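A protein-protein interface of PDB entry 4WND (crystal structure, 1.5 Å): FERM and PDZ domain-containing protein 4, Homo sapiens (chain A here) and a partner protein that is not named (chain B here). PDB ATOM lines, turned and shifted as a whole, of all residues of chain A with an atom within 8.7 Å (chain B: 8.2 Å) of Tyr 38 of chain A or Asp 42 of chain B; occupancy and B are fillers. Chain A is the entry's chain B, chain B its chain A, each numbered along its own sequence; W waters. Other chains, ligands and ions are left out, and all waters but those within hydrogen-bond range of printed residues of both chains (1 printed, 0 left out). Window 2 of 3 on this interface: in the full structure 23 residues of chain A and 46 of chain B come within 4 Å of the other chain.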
ATOM      1  N   SER A  34      24.714  15.357  14.349  1.00  0.00           N
ATOM      2  CA  SER A  34      25.364  15.393  15.651  1.00  0.00           C
ATOM      3  C   SER A  34      24.721  16.493  16.490  1.00  0.00           C
ATOM      4  O   SER A  34      24.347  17.551  15.976  1.00  0.00           O
ATOM      5  CB  SER A  34      26.849  15.693  15.481  1.00  0.00           C
ATOM      6  OG  SER A  34      27.432  15.941  16.752  1.00  0.00           O
ATOM      7  N   VAL A  35      24.587  16.246  17.794  1.00  0.00           N
ATOM      8  CA  VAL A  35      24.150  17.295  18.696  1.00  0.00           C
ATOM      9  C   VAL A  35      25.186  18.441  18.819  1.00  0.00           C
ATOM     10  O   VAL A  35      24.856  19.521  19.270  1.00  0.00           O
ATOM     11  CB  VAL A  35      23.755  16.767  20.088  1.00  0.00           C
ATOM     12  CG1 VAL A  35      22.699  15.678  19.960  1.00  0.00           C
ATOM     13  CG2 VAL A  35      24.993  16.283  20.845  1.00  0.00           C
ATOM     14  N   THR A  36      26.405  18.218  18.333  1.00  0.00           N
ATOM     15  CA  THR A  36      27.406  19.276  18.304  1.00  0.00           C
ATOM     16  C   THR A  36      27.073  20.373  17.300  1.00  0.00           C
ATOM     17  O   THR A  36      27.729  21.417  17.284  1.00  0.00           O
ATOM     18  CB  THR A  36      28.815  18.753  18.032  1.00  0.00           C
ATOM     19  OG1 THR A  36      28.881  18.192  16.715  1.00  0.00           O
ATOM     20  CG2 THR A  36      29.244  17.751  19.070  1.00  0.00           C
ATOM     21  N   ASP A  37      26.048  20.163  16.477  1.00  0.00           N
ATOM     22  CA  ASP A  37      25.580  21.201  15.589  1.00  0.00           C
ATOM     23  C   ASP A  37      24.539  22.138  16.215  1.00  0.00           C
ATOM     24  O   ASP A  37      23.864  22.894  15.508  1.00  0.00           O
ATOM     25  CB  ASP A  37      25.089  20.574  14.280  1.00  0.00           C
ATOM     26  CG  ASP A  37      26.250  20.052  13.420  1.00  0.00           C
ATOM     27  OD1 ASP A  37      27.317  20.733  13.340  1.00  0.00           O
ATOM     28  OD2 ASP A  37      26.139  18.947  12.843  1.00  0.00           O
ATOM     29  N   TYR A  38      24.490  22.148  17.541  1.00  0.00           N
ATOM     30  CA  TYR A  38      23.649  23.050  18.307  1.00  0.00           C
ATOM     31  C   TYR A  38      23.641  24.487  17.830  1.00  0.00           C
ATOM     32  O   TYR A  38      22.572  25.099  17.771  1.00  0.00           O
ATOM     33  CB  TYR A  38      24.059  22.984  19.787  1.00  0.00           C
ATOM     34  CG  TYR A  38      23.197  23.792  20.725  1.00  0.00           C
ATOM     35  CD1 TYR A  38      22.078  23.253  21.318  1.00  0.00           C
ATOM     36  CD2 TYR A  38      23.521  25.104  21.019  1.00  0.00           C
ATOM     37  CE1 TYR A  38      21.290  24.007  22.159  1.00  0.00           C
ATOM     38  CE2 TYR A  38      22.761  25.848  21.893  1.00  0.00           C
ATOM     39  CZ  TYR A  38      21.660  25.299  22.480  1.00  0.00           C
ATOM     40  OH  TYR A  38      20.850  26.070  23.326  1.00  0.00           O
ATOM     41  N   PHE A  39      24.799  25.032  17.511  1.00  0.00           N
ATOM     42  CA  PHE A  39      24.892  26.468  17.175  1.00  0.00           C
ATOM     43  C   PHE A  39      24.596  26.775  15.706  1.00  0.00           C
ATOM     44  O   PHE A  39      24.674  27.931  15.301  1.00  0.00           O
ATOM     45  CB  PHE A  39      26.250  27.037  17.604  1.00  0.00           C
ATOM     46  CG  PHE A  39      26.497  26.912  19.075  1.00  0.00           C
ATOM     47  CD1 PHE A  39      25.912  27.792  19.968  1.00  0.00           C
ATOM     48  CD2 PHE A  39      27.213  25.827  19.588  1.00  0.00           C
ATOM     49  CE1 PHE A  39      26.078  27.633  21.321  1.00  0.00           C
ATOM     50  CE2 PHE A  39      27.394  25.686  20.935  1.00  0.00           C
ATOM     51  CZ  PHE A  39      26.828  26.578  21.807  1.00  0.00           C
ATOM     52  N   SER A  40      24.205  25.763  14.923  1.00  0.00           N
ATOM     53  CA  SER A  40      23.878  25.967  13.483  1.00  0.00           C
ATOM     54  C   SER A  40      22.580  26.752  13.309  1.00  0.00           C
ATOM     55  O   SER A  40      21.677  26.651  14.144  1.00  0.00           O
ATOM     56  CB  SER A  40      23.762  24.613  12.768  1.00  0.00           C
ATOM     57  OG  SER A  40      22.509  23.974  13.039  1.00  0.00           O
ATOM     58  N   LYS A  41      22.476  27.513  12.213  1.00  0.00           N
ATOM     59  CA  LYS A  41      21.251  28.289  11.899  1.00  0.00           C
ATOM     60  C   LYS A  41      20.369  27.544  10.907  1.00  0.00           C
ATOM     61  O   LYS A  41      20.868  26.986   9.928  1.00  0.00           O
ATOM     62  CB  LYS A  41      21.608  29.671  11.328  1.00  0.00           C
ATOM     63  N   CYS B   9      20.376  15.284  28.756  1.00  0.00           N
ATOM     64  CA  CYS B   9      20.094  14.749  27.425  1.00  0.00           C
ATOM     65  C   CYS B   9      21.307  14.951  26.496  1.00  0.00           C
ATOM     66  O   CYS B   9      21.778  13.991  25.870  1.00  0.00           O
ATOM     67  CB  CYS B   9      18.853  15.416  26.828  1.00  0.00           C
ATOM     68  SG  CYS B   9      18.431  14.809  25.183  1.00  0.00           S
ATOM     69  N   LEU B  10      21.787  16.178  26.413  1.00  0.00           N
ATOM     70  CA  LEU B  10      22.936  16.489  25.559  1.00  0.00           C
ATOM     71  C   LEU B  10      24.172  15.682  25.963  1.00  0.00           C
ATOM     72  O   LEU B  10      24.863  15.120  25.114  1.00  0.00           O
ATOM     73  CB  LEU B  10      23.231  17.983  25.605  1.00  0.00           C
ATOM     74  CG  LEU B  10      24.201  18.494  24.565  1.00  0.00           C
ATOM     75  CD1 LEU B  10      23.541  18.635  23.202  1.00  0.00           C
ATOM     76  CD2 LEU B  10      24.766  19.824  25.037  1.00  0.00           C
ATOM     77  N   GLY B  39      14.905  13.003  27.557  1.00  0.00           N
ATOM     78  CA  GLY B  39      14.184  13.881  26.666  1.00  0.00           C
ATOM     79  C   GLY B  39      14.721  15.305  26.624  1.00  0.00           C
ATOM     80  O   GLY B  39      15.542  15.720  27.464  1.00  0.00           O
ATOM     81  N   THR B  40      14.214  16.073  25.661  1.00  0.00           N
ATOM     82  CA  THR B  40      14.535  17.479  25.514  1.00  0.00           C
ATOM     83  C   THR B  40      13.432  18.151  24.713  1.00  0.00           C
ATOM     84  O   THR B  40      12.746  17.476  23.920  1.00  0.00           O
ATOM     85  CB  THR B  40      15.882  17.682  24.765  1.00  0.00           C
ATOM     86  OG1 THR B  40      16.168  19.076  24.653  1.00  0.00           O
ATOM     87  CG2 THR B  40      15.875  17.032  23.346  1.00  0.00           C
ATOM     88  N   GLU B  41      13.297  19.454  24.867  1.00  0.00           N
ATOM     89  CA  GLU B  41      12.357  20.215  24.061  1.00  0.00           C
ATOM     90  C   GLU B  41      13.020  20.812  22.833  1.00  0.00           C
ATOM     91  O   GLU B  41      12.336  21.355  21.963  1.00  0.00           O
ATOM     92  CB  GLU B  41      11.670  21.314  24.873  1.00  0.00           C
ATOM     93  CG  GLU B  41      10.914  20.795  26.106  1.00  0.00           C
ATOM     94  CD  GLU B  41       9.986  19.634  25.808  1.00  0.00           C
ATOM     95  OE1 GLU B  41       8.965  19.843  25.118  1.00  0.00           O
ATOM     96  OE2 GLU B  41      10.239  18.519  26.309  1.00  0.00           O
ATOM     97  N   ASP B  42      14.354  20.650  22.712  1.00  0.00           N
ATOM     98  CA  ASP B  42      15.079  21.126  21.567  1.00  0.00           C
ATOM     99  C   ASP B  42      14.930  20.117  20.431  1.00  0.00           C
ATOM    100  O   ASP B  42      15.560  19.035  20.461  1.00  0.00           O
ATOM    101  CB  ASP B  42      16.533  21.285  21.925  1.00  0.00           C
ATOM    102  CG  ASP B  42      17.325  21.922  20.834  1.00  0.00           C
ATOM    103  OD1 ASP B  42      17.015  21.680  19.631  1.00  0.00           O
ATOM    104  OD2 ASP B  42      18.240  22.695  21.171  1.00  0.00           O
ATOM    105  N   LEU B  43      14.104  20.452  19.457  1.00  0.00           N
ATOM    106  CA  LEU B  43      13.719  19.507  18.463  1.00  0.00           C
ATOM    107  C   LEU B  43      14.866  19.170  17.491  1.00  0.00           C
ATOM    108  O   LEU B  43      14.960  18.031  17.003  1.00  0.00           O
ATOM    109  CB  LEU B  43      12.498  20.019  17.702  1.00  0.00           C
ATOM    110  CG  LEU B  43      11.251  20.251  18.550  1.00  0.00           C
ATOM    111  CD1 LEU B  43      10.176  20.750  17.627  1.00  0.00           C
ATOM    112  CD2 LEU B  43      10.834  18.973  19.263  1.00  0.00           C
ATOM    113  N   LYS B  44      15.753  20.124  17.256  1.00  0.00           N
ATOM    114  CA  LYS B  44      16.938  19.857  16.409  1.00  0.00           C
ATOM    115  C   LYS B  44      17.848  18.819  17.085  1.00  0.00           C
ATOM    116  O   LYS B  44      18.333  17.892  16.451  1.00  0.00           O
ATOM    117  CB  LYS B  44      17.692  21.124  16.118  1.00  0.00           C
ATOM    118  CG  LYS B  44      18.786  20.944  15.081  1.00  0.00           C
ATOM    119  CD  LYS B  44      19.464  22.262  14.714  1.00  0.00           C
ATOM    120  CE  LYS B  44      20.496  22.632  15.750  1.00  0.00           C
ATOM    121  NZ  LYS B  44      20.984  24.030  15.602  1.00  0.00           N
ATOM    122  N   THR B  45      18.099  19.002  18.384  1.00  0.00           N
ATOM    123  CA  THR B  45      18.858  18.045  19.124  1.00  0.00           C
ATOM    124  C   THR B  45      18.181  16.667  19.112  1.00  0.00           C
ATOM    125  O   THR B  45      18.832  15.668  18.873  1.00  0.00           O
ATOM    126  CB  THR B  45      19.042  18.529  20.564  1.00  0.00           C
ATOM    127  OG1 THR B  45      19.803  19.743  20.533  1.00  0.00           O
ATOM    128  CG2 THR B  45      19.706  17.485  21.439  1.00  0.00           C
ATOM    129  N   LEU B  46      16.867  16.627  19.324  1.00  0.00           N
ATOM    130  CA  LEU B  46      16.130  15.383  19.337  1.00  0.00           C
ATOM    131  C   LEU B  46      16.268  14.661  17.987  1.00  0.00           C
ATOM    132  O   LEU B  46      16.499  13.449  17.924  1.00  0.00           O
ATOM    133  CB  LEU B  46      14.674  15.647  19.662  1.00  0.00           C
ATOM    134  CG  LEU B  46      13.819  14.470  19.976  1.00  0.00           C
ATOM    135  CD1 LEU B  46      14.474  13.585  21.053  1.00  0.00           C
ATOM    136  CD2 LEU B  46      12.434  14.968  20.413  1.00  0.00           C
ATOM    137  N   SER B  47      16.127  15.423  16.914  1.00  0.00           N
ATOM    138  CA  SER B  47      16.293  14.826  15.570  1.00  0.00           C
ATOM    139  C   SER B  47      17.685  14.262  15.357  1.00  0.00           C
ATOM    140  O   SER B  47      17.815  13.168  14.830  1.00  0.00           O
ATOM    141  CB  SER B  47      15.878  15.778  14.418  1.00  0.00           C
ATOM    142  OG  SER B  47      16.753  16.874  14.235  1.00  0.00           O
ATOM    143  N   ALA B  48      18.714  14.951  15.834  1.00  0.00           N
ATOM    144  CA  ALA B  48      20.062  14.387  15.728  1.00  0.00           C
ATOM    145  C   ALA B  48      20.234  13.080  16.510  1.00  0.00           C
ATOM    146  O   ALA B  48      20.942  12.167  16.085  1.00  0.00           O
ATOM    147  CB  ALA B  48      21.095  15.416  16.181  1.00  0.00           C
ATOM    148  N   ILE B  49      19.616  13.007  17.688  1.00  0.00           N
ATOM    149  CA  ILE B  49      19.631  11.777  18.491  1.00  0.00           C
ATOM    150  C   ILE B  49      18.926  10.641  17.766  1.00  0.00           C
ATOM    151  O   ILE B  49      19.463   9.549  17.643  1.00  0.00           O
ATOM    152  CB  ILE B  49      19.018  12.014  19.888  1.00  0.00           C
ATOM    153  CG1 ILE B  49      19.900  12.996  20.680  1.00  0.00           C
ATOM    154  CG2 ILE B  49      18.898  10.690  20.667  1.00  0.00           C
ATOM    155  CD1 ILE B  49      19.261  13.576  21.906  1.00  0.00           C
ATOM    156  N   LEU B  76      10.458  15.209  12.537  1.00  0.00           N
ATOM    157  CA  LEU B  76      10.913  16.423  13.180  1.00  0.00           C
ATOM    158  C   LEU B  76      11.589  17.352  12.220  1.00  0.00           C
ATOM    159  O   LEU B  76      11.436  18.567  12.300  1.00  0.00           O
ATOM    160  CB  LEU B  76      11.873  16.117  14.354  1.00  0.00           C
ATOM    161  CG  LEU B  76      11.240  15.466  15.569  1.00  0.00           C
ATOM    162  CD1 LEU B  76      12.313  15.132  16.589  1.00  0.00           C
ATOM    163  CD2 LEU B  76      10.182  16.418  16.112  1.00  0.00           C
ATOM    164  N   ILE B  80      10.281  21.402  11.692  1.00  0.00           N
ATOM    165  CA  ILE B  80      11.103  22.568  12.017  1.00  0.00           C
ATOM    166  C   ILE B  80      11.670  23.235  10.772  1.00  0.00           C
ATOM    167  O   ILE B  80      12.396  24.237  10.861  1.00  0.00           O
ATOM    168  CB  ILE B  80      12.237  22.258  13.043  1.00  0.00           C
ATOM    169  CG1 ILE B  80      13.329  21.386  12.400  1.00  0.00           C
ATOM    170  CG2 ILE B  80      11.660  21.629  14.310  1.00  0.00           C
ATOM    171  CD1 ILE B  80      14.461  21.016  13.350  1.00  0.00           C
HETATM  172  O   HOH W   1      22.024  20.007  18.874  1.00  0.00           O
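Of the 8 printed residues of chain A, 5 touch a printed residue of chain B.
Hydrophobic or aromatic side chains of chain A that line the printed part of chain B: Val 35 and Tyr 38.
Hydrophobic or aromatic side chains of chain B that line the printed part of chain A: Leu 10, Ala 48 and Ile 49.
Among the printed residues, 9 pairs touch across the chains.
Among the printed residues, no Asp or Glu carboxylate lies within 4 Å of a Lys or Arg side-chain nitrogen of the other chain.
Of the printed residues of chain B, Val 35 of chain A touches Leu 10 (3.6 Å), Thr 45 (3.8 Å), Ala 48 (3.9 Å) and Ile 49 (3.9 Å).
Of the printed residues of chain B, Tyr 38 of chain A touches Asp 42 and Lys 44.
Printed residues of chain A within 4 Å of Leu 10 of chain B: Val 35 (3.6 Å).
Leu 43 of chain B touches none of the printed residues of chain A.
Printed residues of chain A within 4 Å of Lys 44 of chain B: Asp 37, Tyr 38 and Ser 40.
Ser 47 of chain B touches none of the printed residues of chain A.
The backbone carbonyl oxygen (O) of Asp 37 of chain A lies within hydrogen-bond range of the side-chain hydroxyl (OG) of Ser 40 of chain A.
The side-chain hydroxyl (OG1) of Thr 40 of chain B is in hydrogen-bond range of the backbone NH (N) of Asp 42 of chain B (3.1 Å).
The side-chain hydroxyl (OG1) of Thr 36 of chain A is in hydrogen-bond range of the side-chain hydroxyl (OG) of Ser 34 of chain A (2.7 Å).
The side-chain carboxylate (OD1) of Asp 42 of chain B is in hydrogen-bond range of the backbone NH (N) of Lys 44 of chain B.
OG of Ser 47 of chain B is in hydrogen-bond range of O of Lys 44 of chain B, 2.9 Å away.
The side-chain carboxylate (OD1) of Asp 42 of chain B sits at hydrogen-bond distance from the backbone NH (N) of Thr 45 of chain B (3.1 Å).
Water W1 lies within hydrogen-bond range of OG1 of Thr 45 of chain B (2.8 Å) and O of Val 35 of chain A (2.9 Å).
Ser 34 of chain A touches Ala 48 of chain B.
Val 35 of chain A touches Leu 10 of chain B.
Thr 45 of chain B touches Val 35 of chain A.
Val 35 of chain A touches Ala 48 of chain B (N to CB, 3.9 Å).
Ile 49 of chain B touches Val 35 of chain A.
Tyr 38 of chain A touches Asp 42 of chain B (CE1 to OD2, 3.5 Å).
O of Tyr 38 of chain A sits at hydrogen-bond distance from NZ of Lys 44 of chain B.
OG of Ser 40 of chain A lies within hydrogen-bond range of NZ of Lys 44 of chain B (3.0 Å).
The side-chain amino group of Lys 44 of chain B lies within hydrogen-bond range of the backbone carbonyl oxygen of Asp 37 of chain A.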
